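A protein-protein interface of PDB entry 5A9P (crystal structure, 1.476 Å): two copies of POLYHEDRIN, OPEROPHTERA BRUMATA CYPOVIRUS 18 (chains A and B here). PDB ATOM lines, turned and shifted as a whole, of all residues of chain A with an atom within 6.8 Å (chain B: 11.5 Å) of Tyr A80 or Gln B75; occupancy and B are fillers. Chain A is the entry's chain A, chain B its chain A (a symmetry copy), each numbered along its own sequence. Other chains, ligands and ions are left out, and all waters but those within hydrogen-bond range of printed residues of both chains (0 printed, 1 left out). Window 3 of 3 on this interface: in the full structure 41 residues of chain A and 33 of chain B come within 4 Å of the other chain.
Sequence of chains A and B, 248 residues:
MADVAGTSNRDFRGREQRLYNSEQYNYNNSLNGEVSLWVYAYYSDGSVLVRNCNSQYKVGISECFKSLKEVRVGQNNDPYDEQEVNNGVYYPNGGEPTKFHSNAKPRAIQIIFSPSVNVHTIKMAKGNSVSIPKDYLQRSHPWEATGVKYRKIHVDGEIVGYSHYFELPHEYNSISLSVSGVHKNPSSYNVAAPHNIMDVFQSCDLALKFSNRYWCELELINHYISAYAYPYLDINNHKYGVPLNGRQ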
ATOM      1  N   ASN A  77      25.948  12.996 -15.121  1.00  0.00           N
ATOM      2  CA  ASN A  77      25.010  11.891 -15.250  1.00  0.00           C
ATOM      3  C   ASN A  77      24.897  11.394 -16.693  1.00  0.00           C
ATOM      4  O   ASN A  77      24.001  10.603 -17.003  1.00  0.00           O
ATOM      5  CB  ASN A  77      23.634  12.314 -14.738  1.00  0.00           C
ATOM      6  CG  ASN A  77      23.634  12.606 -13.253  1.00  0.00           C
ATOM      7  OD1 ASN A  77      23.669  11.689 -12.431  1.00  0.00           O
ATOM      8  ND2 ASN A  77      23.598  13.886 -12.899  1.00  0.00           N
ATOM      9  N   ASP A  78      25.797  11.858 -17.564  1.00  0.00           N
ATOM     10  CA  ASP A  78      25.792  11.466 -18.979  1.00  0.00           C
ATOM     11  C   ASP A  78      24.371  11.465 -19.549  1.00  0.00           C
ATOM     12  O   ASP A  78      23.888  10.433 -20.013  1.00  0.00           O
ATOM     13  CB  ASP A  78      26.403  10.067 -19.143  1.00  0.00           C
ATOM     14  CG  ASP A  78      27.908  10.049 -18.923  1.00  0.00           C
ATOM     15  OD1 ASP A  78      28.547  11.111 -19.051  1.00  0.00           O
ATOM     16  OD2 ASP A  78      28.455   8.961 -18.639  1.00  0.00           O
ATOM     17  N   PRO A  79      23.688  12.618 -19.504  1.00  0.00           N
ATOM     18  CA  PRO A  79      22.249  12.613 -19.800  1.00  0.00           C
ATOM     19  C   PRO A  79      21.882  12.123 -21.201  1.00  0.00           C
ATOM     20  O   PRO A  79      20.863  11.450 -21.319  1.00  0.00           O
ATOM     21  CB  PRO A  79      21.827  14.076 -19.585  1.00  0.00           C
ATOM     22  CG  PRO A  79      23.091  14.868 -19.598  1.00  0.00           C
ATOM     23  CD  PRO A  79      24.173  13.952 -19.111  1.00  0.00           C
ATOM     24  N   TYR A  80      22.672  12.434 -22.226  1.00  0.00           N
ATOM     25  CA  TYR A  80      22.363  11.931 -23.562  1.00  0.00           C
ATOM     26  C   TYR A  80      22.485  10.405 -23.602  1.00  0.00           C
ATOM     27  O   TYR A  80      21.583   9.713 -24.069  1.00  0.00           O
ATOM     28  CB  TYR A  80      23.255  12.558 -24.640  1.00  0.00           C
ATOM     29  CG  TYR A  80      22.882  12.090 -26.031  1.00  0.00           C
ATOM     30  CD1 TYR A  80      21.880  12.727 -26.751  1.00  0.00           C
ATOM     31  CD2 TYR A  80      23.515  10.999 -26.613  1.00  0.00           C
ATOM     32  CE1 TYR A  80      21.526  12.298 -28.013  1.00  0.00           C
ATOM     33  CE2 TYR A  80      23.160  10.555 -27.879  1.00  0.00           C
ATOM     34  CZ  TYR A  80      22.168  11.211 -28.573  1.00  0.00           C
ATOM     35  OH  TYR A  80      21.808  10.786 -29.833  1.00  0.00           O
ATOM     36  N   ASP A  81      23.596   9.885 -23.096  1.00  0.00           N
ATOM     37  CA  ASP A  81      23.816   8.445 -23.078  1.00  0.00           C
ATOM     38  C   ASP A  81      22.704   7.742 -22.291  1.00  0.00           C
ATOM     39  O   ASP A  81      22.252   6.667 -22.671  1.00  0.00           O
ATOM     40  CB  ASP A  81      25.188   8.130 -22.477  1.00  0.00           C
ATOM     41  CG  ASP A  81      25.751   6.792 -22.943  1.00  0.00           C
ATOM     42  OD1 ASP A  81      25.523   6.404 -24.112  1.00  0.00           O
ATOM     43  OD2 ASP A  81      26.450   6.136 -22.142  1.00  0.00           O
ATOM     44  N   GLU A  82      22.252   8.353 -21.199  1.00  0.00           N
ATOM     45  CA  GLU A  82      21.200   7.750 -20.385  1.00  0.00           C
ATOM     46  C   GLU A  82      19.817   7.856 -21.036  1.00  0.00           C
ATOM     47  O   GLU A  82      18.944   7.041 -20.761  1.00  0.00           O
ATOM     48  CB  GLU A  82      21.195   8.345 -18.973  1.00  0.00           C
ATOM     49  CG  GLU A  82      22.331   7.822 -18.093  1.00  0.00           C
ATOM     50  CD  GLU A  82      22.206   6.334 -17.768  1.00  0.00           C
ATOM     51  OE1 GLU A  82      21.098   5.777 -17.902  1.00  0.00           O
ATOM     52  OE2 GLU A  82      23.223   5.721 -17.380  1.00  0.00           O
ATOM     53  N   GLN A  83      19.611   8.845 -21.900  1.00  0.00           N
ATOM     54  CA  GLN A  83      18.392   8.870 -22.705  1.00  0.00           C
ATOM     55  C   GLN A  83      18.423   7.722 -23.708  1.00  0.00           C
ATOM     56  O   GLN A  83      17.389   7.116 -24.013  1.00  0.00           O
ATOM     57  CB  GLN A  83      18.221  10.206 -23.433  1.00  0.00           C
ATOM     58  CG  GLN A  83      17.028  10.247 -24.396  1.00  0.00           C
ATOM     59  CD  GLN A  83      15.704   9.914 -23.724  1.00  0.00           C
ATOM     60  OE1 GLN A  83      15.547  10.076 -22.512  1.00  0.00           O
ATOM     61  NE2 GLN A  83      14.747   9.433 -24.508  1.00  0.00           N
ATOM     62  N   GLU A  84      19.609   7.419 -24.224  1.00  0.00           N
ATOM     63  CA  GLU A  84      19.757   6.285 -25.128  1.00  0.00           C
ATOM     64  C   GLU A  84      19.548   4.958 -24.391  1.00  0.00           C
ATOM     65  O   GLU A  84      18.991   4.015 -24.955  1.00  0.00           O
ATOM     66  CB  GLU A  84      21.111   6.329 -25.838  1.00  0.00           C
ATOM     67  CG  GLU A  84      21.188   7.404 -26.917  1.00  0.00           C
ATOM     68  CD  GLU A  84      20.104   7.246 -27.971  1.00  0.00           C
ATOM     69  OE1 GLU A  84      19.987   6.145 -28.543  1.00  0.00           O
ATOM     70  OE2 GLU A  84      19.349   8.211 -28.209  1.00  0.00           O
ATOM     71  N   VAL A  85      19.975   4.891 -23.133  1.00  0.00           N
ATOM     72  CA  VAL A  85      19.638   3.757 -22.283  1.00  0.00           C
ATOM     73  C   VAL A  85      18.121   3.609 -22.211  1.00  0.00           C
ATOM     74  O   VAL A  85      17.588   2.515 -22.416  1.00  0.00           O
ATOM     75  CB  VAL A  85      20.225   3.925 -20.852  1.00  0.00           C
ATOM     76  CG1 VAL A  85      19.599   2.928 -19.869  1.00  0.00           C
ATOM     77  CG2 VAL A  85      21.731   3.764 -20.886  1.00  0.00           C
ATOM     78  N   ASN A  87      15.793   4.665 -24.280  1.00  0.00           N
ATOM     79  CA  ASN A  87      15.283   4.187 -25.557  1.00  0.00           C
ATOM     80  C   ASN A  87      15.554   2.692 -25.733  1.00  0.00           C
ATOM     81  O   ASN A  87      14.718   1.955 -26.269  1.00  0.00           O
ATOM     82  CB  ASN A  87      15.890   4.996 -26.713  1.00  0.00           C
ATOM     83  CG  ASN A  87      15.286   6.389 -26.834  1.00  0.00           C
ATOM     84  OD1 ASN A  87      14.106   6.586 -26.559  1.00  0.00           O
ATOM     85  ND2 ASN A  87      16.094   7.357 -27.251  1.00  0.00           N
ATOM     86  N   GLU A  96      21.173   3.631 -28.665  1.00  0.00           N
ATOM     87  CA  GLU A  96      22.602   3.452 -28.911  1.00  0.00           C
ATOM     88  C   GLU A  96      23.432   4.051 -27.779  1.00  0.00           C
ATOM     89  O   GLU A  96      24.269   4.933 -27.995  1.00  0.00           O
ATOM     90  CB  GLU A  96      22.987   4.071 -30.253  1.00  0.00           C
ATOM     91  CG  GLU A  96      22.146   5.282 -30.595  1.00  0.00           C
ATOM     92  CD  GLU A  96      22.621   6.004 -31.843  1.00  0.00           C
ATOM     93  OE1 GLU A  96      23.716   5.670 -32.344  1.00  0.00           O
ATOM     94  OE2 GLU A  96      21.897   6.909 -32.315  1.00  0.00           O
ATOM     95  N   PRO A  97      23.208   3.569 -26.553  1.00  0.00           N
ATOM     96  CA  PRO A  97      24.058   4.011 -25.452  1.00  0.00           C
ATOM     97  C   PRO A  97      25.397   3.283 -25.492  1.00  0.00           C
ATOM     98  O   PRO A  97      25.524   2.275 -26.196  1.00  0.00           O
ATOM     99  CB  PRO A  97      23.260   3.597 -24.225  1.00  0.00           C
ATOM    100  CG  PRO A  97      22.595   2.353 -24.651  1.00  0.00           C
ATOM    101  CD  PRO A  97      22.239   2.553 -26.111  1.00  0.00           C
ATOM    102  N   TYR B  43       6.548  18.233 -32.826  1.00  0.00           N
ATOM    103  CA  TYR B  43       7.449  19.366 -33.026  1.00  0.00           C
ATOM    104  C   TYR B  43       7.894  19.498 -34.482  1.00  0.00           C
ATOM    105  O   TYR B  43       7.843  18.536 -35.257  1.00  0.00           O
ATOM    106  CB  TYR B  43       8.670  19.235 -32.122  1.00  0.00           C
ATOM    107  CG  TYR B  43       8.297  19.025 -30.681  1.00  0.00           C
ATOM    108  CD1 TYR B  43       7.605  19.998 -29.979  1.00  0.00           C
ATOM    109  CD2 TYR B  43       8.635  17.852 -30.019  1.00  0.00           C
ATOM    110  CE1 TYR B  43       7.249  19.806 -28.661  1.00  0.00           C
ATOM    111  CE2 TYR B  43       8.289  17.656 -28.710  1.00  0.00           C
ATOM    112  CZ  TYR B  43       7.604  18.639 -28.030  1.00  0.00           C
ATOM    113  OH  TYR B  43       7.260  18.443 -26.712  1.00  0.00           O
ATOM    114  N   ASP B  45      10.749  19.672 -35.820  1.00  0.00           N
ATOM    115  CA  ASP B  45      11.862  18.821 -36.254  1.00  0.00           C
ATOM    116  C   ASP B  45      11.438  17.377 -36.497  1.00  0.00           C
ATOM    117  O   ASP B  45      12.274  16.515 -36.754  1.00  0.00           O
ATOM    118  CB  ASP B  45      13.064  18.874 -35.293  1.00  0.00           C
ATOM    119  CG  ASP B  45      12.748  18.379 -33.890  1.00  0.00           C
ATOM    120  OD1 ASP B  45      11.708  17.717 -33.659  1.00  0.00           O
ATOM    121  OD2 ASP B  45      13.588  18.649 -33.004  1.00  0.00           O
ATOM    122  N   SER B  47      10.068  15.331 -34.371  1.00  0.00           N
ATOM    123  CA  SER B  47      10.004  14.518 -33.160  1.00  0.00           C
ATOM    124  C   SER B  47       8.635  14.646 -32.503  1.00  0.00           C
ATOM    125  O   SER B  47       7.860  15.555 -32.824  1.00  0.00           O
ATOM    126  CB  SER B  47      11.141  14.857 -32.180  1.00  0.00           C
ATOM    127  OG  SER B  47      11.056  16.166 -31.643  1.00  0.00           O
ATOM    128  N   VAL B  48       8.339  13.714 -31.604  1.00  0.00           N
ATOM    129  CA  VAL B  48       7.030  13.631 -30.970  1.00  0.00           C
ATOM    130  C   VAL B  48       7.206  13.267 -29.508  1.00  0.00           C
ATOM    131  O   VAL B  48       7.771  12.217 -29.182  1.00  0.00           O
ATOM    132  CB  VAL B  48       6.141  12.557 -31.621  1.00  0.00           C
ATOM    133  CG1 VAL B  48       4.715  12.659 -31.092  1.00  0.00           C
ATOM    134  CG2 VAL B  48       6.164  12.684 -33.133  1.00  0.00           C
ATOM    135  N   GLU B  70       9.404  21.155 -26.482  1.00  0.00           N
ATOM    136  CA  GLU B  70      10.413  20.158 -26.788  1.00  0.00           C
ATOM    137  C   GLU B  70      11.634  20.289 -25.885  1.00  0.00           C
ATOM    138  O   GLU B  70      12.207  21.373 -25.734  1.00  0.00           O
ATOM    139  CB  GLU B  70      10.855  20.260 -28.246  1.00  0.00           C
ATOM    140  CG  GLU B  70      11.869  19.194 -28.619  1.00  0.00           C
ATOM    141  CD  GLU B  70      12.303  19.261 -30.063  1.00  0.00           C
ATOM    142  OE1 GLU B  70      11.983  20.256 -30.745  1.00  0.00           O
ATOM    143  OE2 GLU B  70      12.966  18.305 -30.517  1.00  0.00           O
ATOM    144  N   VAL B  71      12.021  19.168 -25.292  1.00  0.00           N
ATOM    145  CA  VAL B  71      13.273  19.072 -24.563  1.00  0.00           C
ATOM    146  C   VAL B  71      14.068  17.918 -25.149  1.00  0.00           C
ATOM    147  O   VAL B  71      13.629  16.767 -25.132  1.00  0.00           O
ATOM    148  CB  VAL B  71      13.041  18.849 -23.058  1.00  0.00           C
ATOM    149  CG1 VAL B  71      14.372  18.670 -22.328  1.00  0.00           C
ATOM    150  CG2 VAL B  71      12.261  20.010 -22.468  1.00  0.00           C
ATOM    151  N   ARG B  72      15.230  18.244 -25.694  1.00  0.00           N
ATOM    152  CA  ARG B  72      16.136  17.236 -26.217  1.00  0.00           C
ATOM    153  C   ARG B  72      17.094  16.852 -25.103  1.00  0.00           C
ATOM    154  O   ARG B  72      18.057  17.567 -24.821  1.00  0.00           O
ATOM    155  CB  ARG B  72      16.895  17.790 -27.419  1.00  0.00           C
ATOM    156  CG  ARG B  72      15.987  18.344 -28.505  1.00  0.00           C
ATOM    157  CD  ARG B  72      16.768  18.638 -29.774  1.00  0.00           C
ATOM    158  NE  ARG B  72      17.846  19.594 -29.539  1.00  0.00           N
ATOM    159  CZ  ARG B  72      18.913  19.730 -30.321  1.00  0.00           C
ATOM    160  NH1 ARG B  72      19.053  18.970 -31.402  1.00  0.00           N
ATOM    161  NH2 ARG B  72      19.842  20.628 -30.025  1.00  0.00           N
ATOM    162  N   VAL B  73      16.811  15.733 -24.448  1.00  0.00           N
ATOM    163  CA  VAL B  73      17.590  15.328 -23.287  1.00  0.00           C
ATOM    164  C   VAL B  73      19.055  15.148 -23.662  1.00  0.00           C
ATOM    165  O   VAL B  73      19.379  14.461 -24.625  1.00  0.00           O
ATOM    166  CB  VAL B  73      17.039  14.033 -22.659  1.00  0.00           C
ATOM    167  CG1 VAL B  73      17.906  13.592 -21.481  1.00  0.00           C
ATOM    168  CG2 VAL B  73      15.602  14.241 -22.199  1.00  0.00           C
ATOM    169  N   GLY B  74      19.934  15.795 -22.904  1.00  0.00           N
ATOM    170  CA  GLY B  74      21.366  15.653 -23.095  1.00  0.00           C
ATOM    171  C   GLY B  74      21.920  16.371 -24.314  1.00  0.00           C
ATOM    172  O   GLY B  74      23.072  16.152 -24.698  1.00  0.00           O
ATOM    173  N   GLN B  75      21.104  17.223 -24.927  1.00  0.00           N
ATOM    174  CA  GLN B  75      21.560  18.074 -26.021  1.00  0.00           C
ATOM    175  C   GLN B  75      21.288  19.526 -25.655  1.00  0.00           C
ATOM    176  O   GLN B  75      20.699  19.801 -24.613  1.00  0.00           O
ATOM    177  CB  GLN B  75      20.852  17.704 -27.326  1.00  0.00           C
ATOM    178  CG  GLN B  75      21.152  16.293 -27.794  1.00  0.00           C
ATOM    179  CD  GLN B  75      20.413  15.929 -29.062  1.00  0.00           C
ATOM    180  OE1 GLN B  75      19.318  15.373 -29.015  1.00  0.00           O
ATOM    181  NE2 GLN B  75      21.015  16.234 -30.206  1.00  0.00           N
ATOM    182  N   ASN B  76      21.725  20.456 -26.494  1.00  0.00           N
ATOM    183  CA  ASN B  76      21.531  21.865 -26.178  1.00  0.00           C
ATOM    184  C   ASN B  76      20.091  22.288 -26.397  1.00  0.00           C
ATOM    185  O   ASN B  76      19.524  22.068 -27.467  1.00  0.00           O
ATOM    186  CB  ASN B  76      22.441  22.774 -26.995  1.00  0.00           C
ATOM    187  CG  ASN B  76      22.204  24.237 -26.679  1.00  0.00           C
ATOM    188  OD1 ASN B  76      22.211  24.636 -25.515  1.00  0.00           O
ATOM    189  ND2 ASN B  76      21.935  25.035 -27.708  1.00  0.00           N
ATOM    190  N   ASN B  77      19.509  22.897 -25.370  1.00  0.00           N
ATOM    191  CA  ASN B  77      18.142  23.394 -25.436  1.00  0.00           C
ATOM    192  C   ASN B  77      18.063  24.903 -25.196  1.00  0.00           C
ATOM    193  O   ASN B  77      16.966  25.440 -25.019  1.00  0.00           O
ATOM    194  CB  ASN B  77      17.274  22.660 -24.415  1.00  0.00           C
ATOM    195  CG  ASN B  77      17.130  21.186 -24.730  1.00  0.00           C
ATOM    196  OD1 ASN B  77      16.396  20.807 -25.643  1.00  0.00           O
ATOM    197  ND2 ASN B  77      17.833  20.347 -23.977  1.00  0.00           N
ATOM    198  N   ASP B  78      19.217  25.574 -25.188  1.00  0.00           N
ATOM    199  CA  ASP B  78      19.277  27.024 -24.961  1.00  0.00           C
ATOM    200  C   ASP B  78      18.347  27.446 -23.822  1.00  0.00           C
ATOM    201  O   ASP B  78      17.439  28.250 -24.026  1.00  0.00           O
ATOM    202  CB  ASP B  78      18.885  27.777 -26.239  1.00  0.00           C
ATOM    203  CG  ASP B  78      19.944  27.689 -27.327  1.00  0.00           C
ATOM    204  OD1 ASP B  78      21.119  27.425 -27.004  1.00  0.00           O
ATOM    205  OD2 ASP B  78      19.602  27.904 -28.511  1.00  0.00           O
ATOM    206  N   PRO B  79      18.556  26.894 -22.617  1.00  0.00           N
ATOM    207  CA  PRO B  79      17.548  27.067 -21.563  1.00  0.00           C
ATOM    208  C   PRO B  79      17.275  28.517 -21.164  1.00  0.00           C
ATOM    209  O   PRO B  79      16.119  28.823 -20.892  1.00  0.00           O
ATOM    210  CB  PRO B  79      18.111  26.254 -20.384  1.00  0.00           C
ATOM    211  CG  PRO B  79      19.553  26.036 -20.695  1.00  0.00           C
ATOM    212  CD  PRO B  79      19.672  26.035 -22.188  1.00  0.00           C
ATOM    213  N   TYR B  80      18.285  29.383 -21.132  1.00  0.00           N
ATOM    214  CA  TYR B  80      18.032  30.784 -20.803  1.00  0.00           C
ATOM    215  C   TYR B  80      17.169  31.441 -21.883  1.00  0.00           C
ATOM    216  O   TYR B  80      16.164  32.083 -21.582  1.00  0.00           O
ATOM    217  CB  TYR B  80      19.329  31.579 -20.610  1.00  0.00           C
ATOM    218  CG  TYR B  80      19.063  33.011 -20.197  1.00  0.00           C
ATOM    219  CD1 TYR B  80      18.879  33.344 -18.862  1.00  0.00           C
ATOM    220  CD2 TYR B  80      18.973  34.025 -21.142  1.00  0.00           C
ATOM    221  CE1 TYR B  80      18.623  34.643 -18.479  1.00  0.00           C
ATOM    222  CE2 TYR B  80      18.708  35.334 -20.768  1.00  0.00           C
ATOM    223  CZ  TYR B  80      18.537  35.636 -19.435  1.00  0.00           C
ATOM    224  OH  TYR B  80      18.280  36.932 -19.047  1.00  0.00           O
ATOM    225  N   GLU B  82      15.170  30.053 -23.913  1.00  0.00           N
ATOM    226  CA  GLU B  82      13.827  29.479 -23.892  1.00  0.00           C
ATOM    227  C   GLU B  82      13.010  29.935 -22.679  1.00  0.00           C
ATOM    228  O   GLU B  82      11.785  29.949 -22.734  1.00  0.00           O
ATOM    229  CB  GLU B  82      13.888  27.950 -23.978  1.00  0.00           C
ATOM    230  CG  GLU B  82      14.209  27.435 -25.381  1.00  0.00           C
ATOM    231  CD  GLU B  82      13.105  27.727 -26.397  1.00  0.00           C
ATOM    232  OE1 GLU B  82      11.959  27.996 -25.984  1.00  0.00           O
ATOM    233  OE2 GLU B  82      13.389  27.690 -27.613  1.00  0.00           O
ATOM    234  N   ALA B 104      10.610  24.838 -30.251  1.00  0.00           N
ATOM    235  CA  ALA B 104      10.232  23.914 -29.192  1.00  0.00           C
ATOM    236  C   ALA B 104       8.722  23.919 -28.954  1.00  0.00           C
ATOM    237  O   ALA B 104       8.210  23.064 -28.244  1.00  0.00           O
ATOM    238  CB  ALA B 104      10.972  24.253 -27.904  1.00  0.00           C
ATOM    239  N   ASN B 212       8.171  10.153 -23.127  1.00  0.00           N
ATOM    240  CA  ASN B 212       9.377  10.077 -23.934  1.00  0.00           C
ATOM    241  C   ASN B 212       9.220  10.889 -25.206  1.00  0.00           C
ATOM    242  O   ASN B 212       8.119  11.009 -25.740  1.00  0.00           O
ATOM    243  CB  ASN B 212       9.700   8.636 -24.320  1.00  0.00           C
ATOM    244  CG  ASN B 212      11.150   8.459 -24.736  1.00  0.00           C
ATOM    245  OD1 ASN B 212      12.063   8.950 -24.069  1.00  0.00           O
ATOM    246  ND2 ASN B 212      11.369   7.759 -25.843  1.00  0.00           N
ATOM    247  N   ARG B 213      10.333  11.433 -25.694  1.00  0.00           N
ATOM    248  CA  ARG B 213      10.349  12.101 -26.986  1.00  0.00           C
ATOM    249  C   ARG B 213      10.998  11.197 -28.021  1.00  0.00           C
ATOM    250  O   ARG B 213      12.190  10.898 -27.940  1.00  0.00           O
ATOM    251  CB  ARG B 213      11.095  13.429 -26.909  1.00  0.00           C
ATOM    252  CG  ARG B 213      10.975  14.252 -28.191  1.00  0.00           C
ATOM    253  CD  ARG B 213      11.792  15.527 -28.111  1.00  0.00           C
ATOM    254  NE  ARG B 213      13.204  15.194 -27.983  1.00  0.00           N
ATOM    255  CZ  ARG B 213      14.048  15.063 -29.000  1.00  0.00           C
ATOM    256  NH1 ARG B 213      13.653  15.287 -30.249  1.00  0.00           N
ATOM    257  NH2 ARG B 213      15.304  14.718 -28.760  1.00  0.00           N
ATOM    258  N   TYR B 214      10.199  10.759 -28.985  1.00  0.00           N
ATOM    259  CA  TYR B 214      10.686   9.937 -30.088  1.00  0.00           C
ATOM    260  C   TYR B 214      11.107  10.829 -31.237  1.00  0.00           C
ATOM    261  O   TYR B 214      10.495  11.868 -31.481  1.00  0.00           O
ATOM    262  CB  TYR B 214       9.597   8.947 -30.527  1.00  0.00           C
ATOM    263  CG  TYR B 214       9.362   7.891 -29.483  1.00  0.00           C
ATOM    264  CD1 TYR B 214      10.122   6.736 -29.463  1.00  0.00           C
ATOM    265  CD2 TYR B 214       8.406   8.062 -28.492  1.00  0.00           C
ATOM    266  CE1 TYR B 214       9.937   5.779 -28.488  1.00  0.00           C
ATOM    267  CE2 TYR B 214       8.210   7.110 -27.515  1.00  0.00           C
ATOM    268  CZ  TYR B 214       8.978   5.968 -27.520  1.00  0.00           C
ATOM    269  OH  TYR B 214       8.798   5.009 -26.549  1.00  0.00           O
ATOM    270  N   TRP B 215      12.157  10.425 -31.945  1.00  0.00           N
ATOM    271  CA  TRP B 215      12.754  11.294 -32.952  1.00  0.00           C
ATOM    272  C   TRP B 215      11.856  11.497 -34.170  1.00  0.00           C
ATOM    273  O   TRP B 215      12.013  12.466 -34.904  1.00  0.00           O
ATOM    274  CB  TRP B 215      14.114  10.760 -33.387  1.00  0.00           C
ATOM    275  CG  TRP B 215      15.194  10.933 -32.363  1.00  0.00           C
ATOM    276  CD1 TRP B 215      15.077  11.464 -31.106  1.00  0.00           C
ATOM    277  CD2 TRP B 215      16.570  10.577 -32.521  1.00  0.00           C
ATOM    278  NE1 TRP B 215      16.301  11.451 -30.473  1.00  0.00           N
ATOM    279  CE2 TRP B 215      17.232  10.914 -31.323  1.00  0.00           C
ATOM    280  CE3 TRP B 215      17.307  10.002 -33.562  1.00  0.00           C
ATOM    281  CZ2 TRP B 215      18.593  10.692 -31.136  1.00  0.00           C
ATOM    282  CZ3 TRP B 215      18.658   9.784 -33.376  1.00  0.00           C
ATOM    283  CH2 TRP B 215      19.286  10.126 -32.171  1.00  0.00           C
ATOM    284  N   CYS B 216      10.918  10.584 -34.396  1.00  0.00           N
ATOM    285  CA  CYS B 216       9.958  10.766 -35.479  1.00  0.00           C
ATOM    286  C   CYS B 216       8.761   9.844 -35.342  1.00  0.00           C
ATOM    287  O   CYS B 216       8.755   8.934 -34.515  1.00  0.00           O
ATOM    288  CB  CYS B 216      10.626  10.588 -36.851  1.00  0.00           C
ATOM    289  SG  CYS B 216      11.219   8.928 -37.220  1.00  0.00           S
ATOM    290  N   GLU B 219       9.386   6.131 -35.752  1.00  0.00           N
ATOM    291  CA  GLU B 219       9.995   5.464 -34.603  1.00  0.00           C
ATOM    292  C   GLU B 219       8.951   5.229 -33.519  1.00  0.00           C
ATOM    293  O   GLU B 219       8.942   4.188 -32.865  1.00  0.00           O
ATOM    294  CB  GLU B 219      11.158   6.289 -34.052  1.00  0.00           C
ATOM    295  CG  GLU B 219      11.958   5.552 -32.993  1.00  0.00           C
ATOM    296  CD  GLU B 219      13.119   6.355 -32.456  1.00  0.00           C
ATOM    297  OE1 GLU B 219      13.804   7.038 -33.251  1.00  0.00           O
ATOM    298  OE2 GLU B 219      13.358   6.279 -31.228  1.00  0.00           O
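Positions printed for both chains: 77, 78, 79, 80 and 82.
Pro A79 touches Val B73 (O to CG1, 3.7 Å). Pro A79 touches Gly B74. Val B73 touches Tyr A80. Gly B74 touches Tyr A80 (CA to N, 3.6 Å). CG of Gln B75 touches CD1 of Tyr A80, 3.8 Å away. OH of Tyr A80 touches CZ2 of Trp B215, 3.5 Å away. CG1 of Val B73 touches CB of Gln A83 (3.9 Å). OE2 of Glu A84 touches CZ2 of Trp B215 (3.9 Å).
Printed residues of chain B that touch a printed residue of chain A: Val B73, Gly B74, Gln B75, Asn B212 and Trp B215. Hydrophobic or aromatic side chains of chain A within 4 Å of the printed part of chain B: Pro A79 and Tyr A80. Along chain A the printed residues that touch a printed residue of chain B span positions 79 to 87. Among the printed residues, 10 pairs touch across the chains.
O of Gln A83 sits at hydrogen-bond distance from ND2 of Asn A87. N of Glu A96 lies within hydrogen-bond range of OE1 of Glu A84, 2.8 Å away. ND2 of Asn A87 lies within hydrogen-bond range of OE2 of Glu A84, 3.5 Å away. The backbone carbonyl oxygen of Gln B75 sits at hydrogen-bond distance from the side-chain amide nitrogen of Asn B77, at 3.0 Å.
Of chain B, only Val B73, Gly B74, Gln B75 and Trp B215 come within 4 Å of Tyr A80. Of chain A, only Tyr A80 (3.8 Å) comes within 4 Å of Gln B75. Pro A79 touches just these residues of chain B: Val B73 (3.7 Å) and Gly B74 (3.9 Å). No residue of chain B comes within 4 Å of Asp A81. No residue of chain B comes within 4 Å of Glu A96. Gly B74 touches just these residues of chain A: Pro A79 and Tyr A80. Printed residues of chain B within 4 Å of Asn A87: Asn B212. Printed residues of chain A within 4 Å of Val B73: Pro A79 (3.7 Å), Tyr A80 (3.7 Å) and Gln A83 (3.9 Å). Printed residues of chain A within 4 Å of Trp B215: Tyr A80 (3.5 Å) and Glu A84 (3.9 Å). Printed residues of chain A within 4 Å of Asn B212: Gln A83 and Asn A87. The nearest residue of chain A that does not touch Gln B75 is Pro A79 (6.2 Å).
The side-chain amide nitrogen of Gln A83 sits at hydrogen-bond distance from the side-chain amide oxygen of Asn B212 (2.8 Å). ND2 of Asn B212 is in hydrogen-bond range of OD1 of Asn A87 (3.1 Å).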
